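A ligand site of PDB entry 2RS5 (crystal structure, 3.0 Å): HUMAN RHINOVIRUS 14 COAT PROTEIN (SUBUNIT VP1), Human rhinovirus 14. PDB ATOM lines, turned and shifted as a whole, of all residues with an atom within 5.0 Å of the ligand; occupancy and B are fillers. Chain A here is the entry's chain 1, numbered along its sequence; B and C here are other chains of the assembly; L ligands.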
ATOM      1  N   ILE A 104      -1.784 -16.371 -18.011  1.00  0.00           N
ATOM      2  CA  ILE A 104      -1.438 -17.127 -19.268  1.00  0.00           C
ATOM      3  C   ILE A 104      -0.043 -16.950 -19.776  1.00  0.00           C
ATOM      4  O   ILE A 104       0.535 -15.868 -19.690  1.00  0.00           O
ATOM      5  CB  ILE A 104      -2.320 -16.712 -20.432  1.00  0.00           C
ATOM      6  CG1 ILE A 104      -3.756 -17.170 -20.277  1.00  0.00           C
ATOM      7  CG2 ILE A 104      -1.881 -17.287 -21.786  1.00  0.00           C
ATOM      8  CD1 ILE A 104      -4.595 -16.866 -21.518  1.00  0.00           C
ATOM      9  N   ASN A 105       0.442 -18.019 -20.357  1.00  0.00           N
ATOM     10  CA  ASN A 105       1.841 -18.085 -20.742  1.00  0.00           C
ATOM     11  C   ASN A 105       2.112 -19.490 -21.294  1.00  0.00           C
ATOM     12  O   ASN A 105       1.391 -20.431 -20.999  1.00  0.00           O
ATOM     13  CB  ASN A 105       2.596 -17.840 -19.453  1.00  0.00           C
ATOM     14  CG  ASN A 105       3.226 -19.112 -18.908  1.00  0.00           C
ATOM     15  OD1 ASN A 105       4.259 -19.521 -19.410  1.00  0.00           O
ATOM     16  ND2 ASN A 105       2.671 -19.772 -17.896  1.00  0.00           N
ATOM     17  N   LEU A 106       3.179 -19.683 -22.062  1.00  0.00           N
ATOM     18  CA  LEU A 106       3.381 -21.016 -22.702  1.00  0.00           C
ATOM     19  C   LEU A 106       4.679 -21.705 -22.254  1.00  0.00           C
ATOM     20  O   LEU A 106       4.823 -22.943 -22.360  1.00  0.00           O
ATOM     21  CB  LEU A 106       3.475 -20.833 -24.215  1.00  0.00           C
ATOM     22  CG  LEU A 106       2.370 -21.574 -24.981  1.00  0.00           C
ATOM     23  CD1 LEU A 106       0.958 -21.082 -24.632  1.00  0.00           C
ATOM     24  CD2 LEU A 106       2.501 -21.408 -26.501  1.00  0.00           C
ATOM     25  N   VAL A 122       8.157 -16.263 -33.288  1.00  0.00           N
ATOM     26  CA  VAL A 122       7.243 -17.428 -33.752  1.00  0.00           C
ATOM     27  C   VAL A 122       5.935 -16.779 -33.940  1.00  0.00           C
ATOM     28  O   VAL A 122       5.666 -15.779 -33.174  1.00  0.00           O
ATOM     29  CB  VAL A 122       7.526 -18.385 -32.590  1.00  0.00           C
ATOM     30  CG1 VAL A 122       6.483 -18.451 -31.556  1.00  0.00           C
ATOM     31  CG2 VAL A 122       7.985 -19.680 -33.169  1.00  0.00           C
ATOM     32  N   PHE A 124       1.688 -17.794 -34.754  1.00  0.00           N
ATOM     33  CA  PHE A 124       0.765 -18.896 -34.995  1.00  0.00           C
ATOM     34  C   PHE A 124      -0.587 -18.614 -34.387  1.00  0.00           C
ATOM     35  O   PHE A 124      -0.681 -17.696 -33.560  1.00  0.00           O
ATOM     36  CB  PHE A 124       1.416 -20.195 -34.514  1.00  0.00           C
ATOM     37  CG  PHE A 124       1.921 -20.168 -33.123  1.00  0.00           C
ATOM     38  CD1 PHE A 124       1.068 -20.085 -32.039  1.00  0.00           C
ATOM     39  CD2 PHE A 124       3.278 -20.287 -32.848  1.00  0.00           C
ATOM     40  CE1 PHE A 124       1.515 -20.085 -30.733  1.00  0.00           C
ATOM     41  CE2 PHE A 124       3.750 -20.255 -31.544  1.00  0.00           C
ATOM     42  CZ  PHE A 124       2.862 -20.130 -30.488  1.00  0.00           C
ATOM     43  N   SER A 126      -3.694 -20.328 -32.078  1.00  0.00           N
ATOM     44  CA  SER A 126      -3.663 -21.368 -31.054  1.00  0.00           C
ATOM     45  C   SER A 126      -4.953 -22.114 -31.068  1.00  0.00           C
ATOM     46  O   SER A 126      -5.993 -21.454 -31.245  1.00  0.00           O
ATOM     47  CB  SER A 126      -3.472 -20.764 -29.685  1.00  0.00           C
ATOM     48  OG  SER A 126      -2.221 -20.031 -29.785  1.00  0.00           O
ATOM     49  N   TYR A 128      -6.888 -24.305 -28.312  1.00  0.00           N
ATOM     50  CA  TYR A 128      -6.839 -24.816 -26.941  1.00  0.00           C
ATOM     51  C   TYR A 128      -7.740 -26.001 -26.724  1.00  0.00           C
ATOM     52  O   TYR A 128      -8.901 -25.941 -27.293  1.00  0.00           O
ATOM     53  CB  TYR A 128      -7.266 -23.726 -25.969  1.00  0.00           C
ATOM     54  CG  TYR A 128      -6.141 -22.720 -25.755  1.00  0.00           C
ATOM     55  CD1 TYR A 128      -6.120 -21.535 -26.491  1.00  0.00           C
ATOM     56  CD2 TYR A 128      -5.136 -23.004 -24.834  1.00  0.00           C
ATOM     57  CE1 TYR A 128      -5.089 -20.626 -26.309  1.00  0.00           C
ATOM     58  CE2 TYR A 128      -4.097 -22.085 -24.645  1.00  0.00           C
ATOM     59  CZ  TYR A 128      -4.063 -20.899 -25.385  1.00  0.00           C
ATOM     60  OH  TYR A 128      -3.062 -20.010 -25.213  1.00  0.00           O
ATOM     61  N   ALA A 150     -14.789 -21.478 -18.061  1.00  0.00           N
ATOM     62  CA  ALA A 150     -13.455 -20.890 -18.211  1.00  0.00           C
ATOM     63  C   ALA A 150     -13.651 -19.577 -18.931  1.00  0.00           C
ATOM     64  O   ALA A 150     -14.291 -19.527 -19.963  1.00  0.00           O
ATOM     65  CB  ALA A 150     -12.598 -21.831 -19.070  1.00  0.00           C
ATOM     66  N   MET A 151     -13.122 -18.499 -18.423  1.00  0.00           N
ATOM     67  CA  MET A 151     -13.376 -17.191 -19.064  1.00  0.00           C
ATOM     68  C   MET A 151     -12.061 -16.466 -19.305  1.00  0.00           C
ATOM     69  O   MET A 151     -11.136 -16.539 -18.502  1.00  0.00           O
ATOM     70  CB  MET A 151     -14.280 -16.386 -18.137  1.00  0.00           C
ATOM     71  CG  MET A 151     -14.082 -14.888 -18.260  1.00  0.00           C
ATOM     72  SD  MET A 151     -15.299 -13.958 -17.344  1.00  0.00           S
ATOM     73  CE  MET A 151     -14.650 -13.495 -15.749  1.00  0.00           C
ATOM     74  N   TYR A 152     -11.959 -15.747 -20.405  1.00  0.00           N
ATOM     75  CA  TYR A 152     -10.716 -15.002 -20.735  1.00  0.00           C
ATOM     76  C   TYR A 152     -10.802 -13.613 -20.134  1.00  0.00           C
ATOM     77  O   TYR A 152     -11.778 -12.898 -20.348  1.00  0.00           O
ATOM     78  CB  TYR A 152     -10.538 -14.873 -22.261  1.00  0.00           C
ATOM     79  CG  TYR A 152      -9.218 -14.203 -22.714  1.00  0.00           C
ATOM     80  CD1 TYR A 152      -9.221 -13.296 -23.796  1.00  0.00           C
ATOM     81  CD2 TYR A 152      -8.010 -14.476 -22.059  1.00  0.00           C
ATOM     82  CE1 TYR A 152      -8.025 -12.690 -24.216  1.00  0.00           C
ATOM     83  CE2 TYR A 152      -6.816 -13.872 -22.488  1.00  0.00           C
ATOM     84  CZ  TYR A 152      -6.823 -12.986 -23.566  1.00  0.00           C
ATOM     85  OH  TYR A 152      -5.658 -12.406 -23.974  1.00  0.00           O
ATOM     86  N   PRO A 174     -14.993 -13.439 -24.095  1.00  0.00           N
ATOM     87  CA  PRO A 174     -15.414 -14.792 -24.566  1.00  0.00           C
ATOM     88  C   PRO A 174     -15.387 -15.756 -23.449  1.00  0.00           C
ATOM     89  O   PRO A 174     -14.345 -15.802 -22.798  1.00  0.00           O
ATOM     90  CB  PRO A 174     -14.434 -15.113 -25.687  1.00  0.00           C
ATOM     91  CG  PRO A 174     -13.329 -14.265 -25.556  1.00  0.00           C
ATOM     92  CD  PRO A 174     -13.638 -13.146 -24.548  1.00  0.00           C
ATOM     93  N   SER A 175     -16.470 -16.492 -23.227  1.00  0.00           N
ATOM     94  CA  SER A 175     -16.291 -17.613 -22.156  1.00  0.00           C
ATOM     95  C   SER A 175     -16.927 -18.873 -22.669  1.00  0.00           C
ATOM     96  O   SER A 175     -17.776 -18.793 -23.618  1.00  0.00           O
ATOM     97  CB  SER A 175     -16.545 -17.005 -20.868  1.00  0.00           C
ATOM     98  OG  SER A 175     -17.700 -17.071 -20.276  1.00  0.00           O
ATOM     99  N   VAL A 176     -16.464 -20.079 -22.320  1.00  0.00           N
ATOM    100  CA  VAL A 176     -16.968 -21.336 -22.732  1.00  0.00           C
ATOM    101  C   VAL A 176     -17.516 -22.097 -21.453  1.00  0.00           C
ATOM    102  O   VAL A 176     -16.666 -22.081 -20.488  1.00  0.00           O
ATOM    103  CB  VAL A 176     -15.896 -22.381 -23.192  1.00  0.00           C
ATOM    104  CG1 VAL A 176     -16.417 -23.198 -24.322  1.00  0.00           C
ATOM    105  CG2 VAL A 176     -14.549 -21.900 -23.286  1.00  0.00           C
ATOM    106  N   PHE A 186     -11.631 -24.581 -28.581  1.00  0.00           N
ATOM    107  CA  PHE A 186     -11.991 -23.363 -29.294  1.00  0.00           C
ATOM    108  C   PHE A 186     -10.616 -22.895 -29.865  1.00  0.00           C
ATOM    109  O   PHE A 186      -9.679 -23.597 -29.444  1.00  0.00           O
ATOM    110  CB  PHE A 186     -12.677 -22.505 -28.204  1.00  0.00           C
ATOM    111  CG  PHE A 186     -11.674 -22.186 -27.131  1.00  0.00           C
ATOM    112  CD1 PHE A 186     -11.677 -22.868 -25.906  1.00  0.00           C
ATOM    113  CD2 PHE A 186     -10.738 -21.221 -27.415  1.00  0.00           C
ATOM    114  CE1 PHE A 186     -10.691 -22.567 -24.951  1.00  0.00           C
ATOM    115  CE2 PHE A 186      -9.743 -20.921 -26.483  1.00  0.00           C
ATOM    116  CZ  PHE A 186      -9.717 -21.598 -25.257  1.00  0.00           C
ATOM    117  N   VAL A 188      -7.933 -19.496 -30.882  1.00  0.00           N
ATOM    118  CA  VAL A 188      -7.826 -17.999 -30.729  1.00  0.00           C
ATOM    119  C   VAL A 188      -6.849 -17.542 -31.789  1.00  0.00           C
ATOM    120  O   VAL A 188      -5.870 -18.292 -32.021  1.00  0.00           O
ATOM    121  CB  VAL A 188      -7.058 -17.822 -29.423  1.00  0.00           C
ATOM    122  CG1 VAL A 188      -6.665 -16.394 -29.124  1.00  0.00           C
ATOM    123  CG2 VAL A 188      -7.783 -18.419 -28.229  1.00  0.00           C
ATOM    124  N   VAL A 191      -2.869 -13.311 -31.079  1.00  0.00           N
ATOM    125  CA  VAL A 191      -3.089 -12.108 -30.371  1.00  0.00           C
ATOM    126  C   VAL A 191      -1.874 -11.273 -30.016  1.00  0.00           C
ATOM    127  O   VAL A 191      -2.069 -10.303 -29.181  1.00  0.00           O
ATOM    128  CB  VAL A 191      -4.034 -12.331 -29.211  1.00  0.00           C
ATOM    129  CG1 VAL A 191      -5.297 -12.866 -29.697  1.00  0.00           C
ATOM    130  CG2 VAL A 191      -3.214 -13.066 -28.229  1.00  0.00           C
ATOM    131  N   TYR A 197       5.629 -13.327 -31.913  1.00  0.00           N
ATOM    132  CA  TYR A 197       5.805 -13.374 -30.432  1.00  0.00           C
ATOM    133  C   TYR A 197       7.302 -13.426 -30.185  1.00  0.00           C
ATOM    134  O   TYR A 197       7.909 -14.199 -31.026  1.00  0.00           O
ATOM    135  CB  TYR A 197       4.927 -14.621 -30.442  1.00  0.00           C
ATOM    136  CG  TYR A 197       3.448 -14.802 -30.331  1.00  0.00           C
ATOM    137  CD1 TYR A 197       2.612 -13.870 -29.738  1.00  0.00           C
ATOM    138  CD2 TYR A 197       2.869 -15.972 -30.769  1.00  0.00           C
ATOM    139  CE1 TYR A 197       1.250 -14.058 -29.583  1.00  0.00           C
ATOM    140  CE2 TYR A 197       1.494 -16.202 -30.646  1.00  0.00           C
ATOM    141  CZ  TYR A 197       0.733 -15.224 -30.059  1.00  0.00           C
ATOM    142  OH  TYR A 197      -0.603 -15.473 -30.017  1.00  0.00           O
ATOM    143  N   ASN A 198       7.882 -12.745 -29.236  1.00  0.00           N
ATOM    144  CA  ASN A 198       9.686 -13.227 -29.503  1.00  0.00           C
ATOM    145  C   ASN A 198       9.712 -14.429 -28.609  1.00  0.00           C
ATOM    146  O   ASN A 198       8.959 -14.494 -27.621  1.00  0.00           O
ATOM    147  CB  ASN A 198       9.965 -11.746 -28.365  1.00  0.00           C
ATOM    148  CG  ASN A 198      10.176 -10.445 -29.140  1.00  0.00           C
ATOM    149  OD1 ASN A 198      11.273  -9.893 -29.126  1.00  0.00           O
ATOM    150  ND2 ASN A 198       9.175  -9.907 -29.821  1.00  0.00           N
ATOM    151  N   CYS A 199      10.491 -15.396 -28.846  1.00  0.00           N
ATOM    152  CA  CYS A 199      10.548 -16.459 -27.867  1.00  0.00           C
ATOM    153  C   CYS A 199      11.474 -15.960 -26.814  1.00  0.00           C
ATOM    154  O   CYS A 199      11.538 -16.492 -25.684  1.00  0.00           O
ATOM    155  CB  CYS A 199      11.073 -17.728 -28.490  1.00  0.00           C
ATOM    156  SG  CYS A 199       9.703 -18.911 -28.902  1.00  0.00           S
ATOM    157  N   ASN A 219       5.499 -10.378 -23.173  1.00  0.00           N
ATOM    158  CA  ASN A 219       4.536 -11.498 -23.223  1.00  0.00           C
ATOM    159  C   ASN A 219       3.458 -11.387 -22.167  1.00  0.00           C
ATOM    160  O   ASN A 219       3.268 -12.309 -21.376  1.00  0.00           O
ATOM    161  CB  ASN A 219       5.281 -12.736 -22.882  1.00  0.00           C
ATOM    162  CG  ASN A 219       5.571 -13.538 -24.095  1.00  0.00           C
ATOM    163  OD1 ASN A 219       5.996 -12.977 -25.108  1.00  0.00           O
ATOM    164  ND2 ASN A 219       5.346 -14.827 -24.062  1.00  0.00           N
ATOM    165  N   MET A 221      -0.459 -10.889 -21.652  1.00  0.00           N
ATOM    166  CA  MET A 221      -1.650 -11.226 -22.484  1.00  0.00           C
ATOM    167  C   MET A 221      -2.886 -11.615 -21.732  1.00  0.00           C
ATOM    168  O   MET A 221      -3.828 -12.185 -22.298  1.00  0.00           O
ATOM    169  CB  MET A 221      -1.412 -12.483 -23.304  1.00  0.00           C
ATOM    170  CG  MET A 221       0.043 -12.863 -23.326  1.00  0.00           C
ATOM    171  SD  MET A 221       0.615 -13.039 -24.991  1.00  0.00           S
ATOM    172  CE  MET A 221      -0.350 -11.974 -26.041  1.00  0.00           C
ATOM    173  N   MET A 224      -6.442 -16.511 -17.697  1.00  0.00           N
ATOM    174  CA  MET A 224      -7.700 -17.210 -17.947  1.00  0.00           C
ATOM    175  C   MET A 224      -8.247 -17.721 -16.616  1.00  0.00           C
ATOM    176  O   MET A 224      -7.523 -18.203 -15.744  1.00  0.00           O
ATOM    177  CB  MET A 224      -7.513 -18.191 -19.145  1.00  0.00           C
ATOM    178  CG  MET A 224      -6.980 -19.578 -18.828  1.00  0.00           C
ATOM    179  SD  MET A 224      -7.599 -20.768 -20.006  1.00  0.00           S
ATOM    180  CE  MET A 224      -6.727 -20.575 -21.540  1.00  0.00           C
ATOM    181  N   HIS A 245      -2.322 -26.968 -25.738  1.00  0.00           N
ATOM    182  CA  HIS A 245      -2.200 -25.928 -26.771  1.00  0.00           C
ATOM    183  C   HIS A 245      -1.595 -26.503 -28.032  1.00  0.00           C
ATOM    184  O   HIS A 245      -0.591 -27.194 -27.945  1.00  0.00           O
ATOM    185  CB  HIS A 245      -1.368 -24.772 -26.283  1.00  0.00           C
ATOM    186  CG  HIS A 245      -0.976 -23.821 -27.363  1.00  0.00           C
ATOM    187  ND1 HIS A 245       0.064 -24.060 -28.241  1.00  0.00           N
ATOM    188  CD2 HIS A 245      -1.497 -22.582 -27.669  1.00  0.00           C
ATOM    189  CE1 HIS A 245       0.149 -22.976 -29.051  1.00  0.00           C
ATOM    190  NE2 HIS A 245      -0.753 -22.096 -28.735  1.00  0.00           N
ATOM    191  N   LEU B  14     -19.977 -21.675 -26.148  1.00  0.00           N
ATOM    192  CA  LEU B  14     -18.922 -20.629 -26.216  1.00  0.00           C
ATOM    193  C   LEU B  14     -19.642 -19.320 -26.418  1.00  0.00           C
ATOM    194  O   LEU B  14     -20.267 -19.206 -27.528  1.00  0.00           O
ATOM    195  CB  LEU B  14     -17.999 -21.054 -27.346  1.00  0.00           C
ATOM    196  CG  LEU B  14     -17.029 -20.030 -27.901  1.00  0.00           C
ATOM    197  CD1 LEU B  14     -16.028 -19.691 -26.778  1.00  0.00           C
ATOM    198  CD2 LEU B  14     -16.271 -20.611 -29.045  1.00  0.00           C
ATOM    199  N   ALA C  24     -12.658 -18.024 -30.670  1.00  0.00           N
ATOM    200  CA  ALA C  24     -13.154 -17.314 -29.491  1.00  0.00           C
ATOM    201  C   ALA C  24     -13.242 -15.801 -29.728  1.00  0.00           C
ATOM    202  O   ALA C  24     -14.110 -15.227 -29.077  1.00  0.00           O
ATOM    203  CB  ALA C  24     -12.281 -17.527 -28.253  1.00  0.00           C
HETATM  204  O1  LIG L   1       2.405 -17.000 -25.412  1.00  0.00           O
HETATM  205  N1  LIG L   1       3.795 -16.831 -25.633  1.00  0.00           N
HETATM  206  C1  LIG L   1       4.054 -17.376 -26.776  1.00  0.00           C
HETATM  207  C2  LIG L   1       5.446 -17.377 -27.315  1.00  0.00           C
HETATM  208  C3  LIG L   1       2.890 -17.901 -27.353  1.00  0.00           C
HETATM  209  C4  LIG L   1       1.887 -17.663 -26.474  1.00  0.00           C
HETATM  210  C5  LIG L   1       0.432 -17.995 -26.439  1.00  0.00           C
HETATM  211  C6  LIG L   1      -0.522 -16.792 -26.414  1.00  0.00           C
HETATM  212  C7  LIG L   1      -2.004 -17.213 -26.535  1.00  0.00           C
HETATM  213  C8  LIG L   1      -2.982 -16.130 -26.924  1.00  0.00           C
HETATM  214  C9  LIG L   1      -4.115 -15.857 -25.891  1.00  0.00           C
HETATM  215  O2  LIG L   1      -4.739 -17.136 -25.544  1.00  0.00           O
HETATM  216  C10 LIG L   1      -6.106 -17.254 -25.169  1.00  0.00           C
HETATM  217  C11 LIG L   1      -7.189 -16.458 -25.598  1.00  0.00           C
HETATM  218  C12 LIG L   1      -8.486 -16.750 -25.203  1.00  0.00           C
HETATM  219  C13 LIG L   1      -8.745 -17.819 -24.349  1.00  0.00           C
HETATM  220  C14 LIG L   1      -7.669 -18.566 -23.874  1.00  0.00           C
HETATM  221  C15 LIG L   1      -6.386 -18.291 -24.273  1.00  0.00           C
HETATM  222  C16 LIG L   1     -10.121 -18.231 -24.018  1.00  0.00           C
HETATM  223  N2  LIG L   1     -11.324 -17.641 -24.507  1.00  0.00           N
HETATM  224  C17 LIG L   1     -12.445 -18.272 -24.040  1.00  0.00           C
HETATM  225  C18 LIG L   1     -13.560 -18.999 -24.680  1.00  0.00           C
HETATM  226  C19 LIG L   1     -11.772 -19.318 -23.177  1.00  0.00           C
HETATM  227  O3  LIG L   1     -10.391 -19.207 -23.218  1.00  0.00           O
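A nitrogen (N1) of the ligand sits at hydrogen-bond distance from the side-chain amide nitrogen of Asn 219 (3.0 Å). OH of Tyr 128 lies close to O2 of the ligand (3.3 Å).
Residues that only touch the ligand: Ile 104 (3.6 Å), Leu 106 (3.6 Å), Phe 124 (3.8 Å), Tyr 152 (3.6 Å), Pro 174 (3.4 Å), Ser 175 (3.9 Å), Val 176 (3.4 Å), Phe 186 (3.2 Å), Val 188 (3.3 Å), Val 191 (3.3 Å), Tyr 197 (3.8 Å), Met 224 (3.2 Å), Leu 14 of chain B (3.3 Å) and Ala 24 of chain C (3.9 Å). Hydrophobic or aromatic side chains within 4 Å of the ligand: Ile 104, Leu 106, Phe 124, Tyr 128, Tyr 152, Val 176, Phe 186, Val 188, Val 191, Tyr 197, Met 224, Leu 14 of chain B and Ala 24 of chain C. 16 residues have an atom within 4 Å of the ligand: Ile 104, Leu 106, Phe 124, Tyr 128, Tyr 152, Pro 174, Ser 175, Val 176, Phe 186, Val 188, Val 191, Tyr 197, Asn 219, Met 224, Leu 14 of chain B and Ala 24 of chain C.
O of Phe 186 sits at hydrogen-bond distance from N of Tyr 128 (3.1 Å). The backbone NH (N) of Val 188 sits at hydrogen-bond distance from the backbone carbonyl oxygen (O) of Ser 126, 2.8 Å away. N of Val 191 lies within hydrogen-bond range of OH of Tyr 197, at 3.3 Å. The backbone NH (N) of Tyr 152 sits at hydrogen-bond distance from the backbone carbonyl oxygen (O) of Pro 174. O of Val 176 sits at hydrogen-bond distance from N of Ala 150 (3.1 Å). OH of Tyr 152 is in hydrogen-bond range of O of Met 221 (2.5 Å). N of Tyr 197 lies within hydrogen-bond range of O of Val 122 (2.8 Å).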
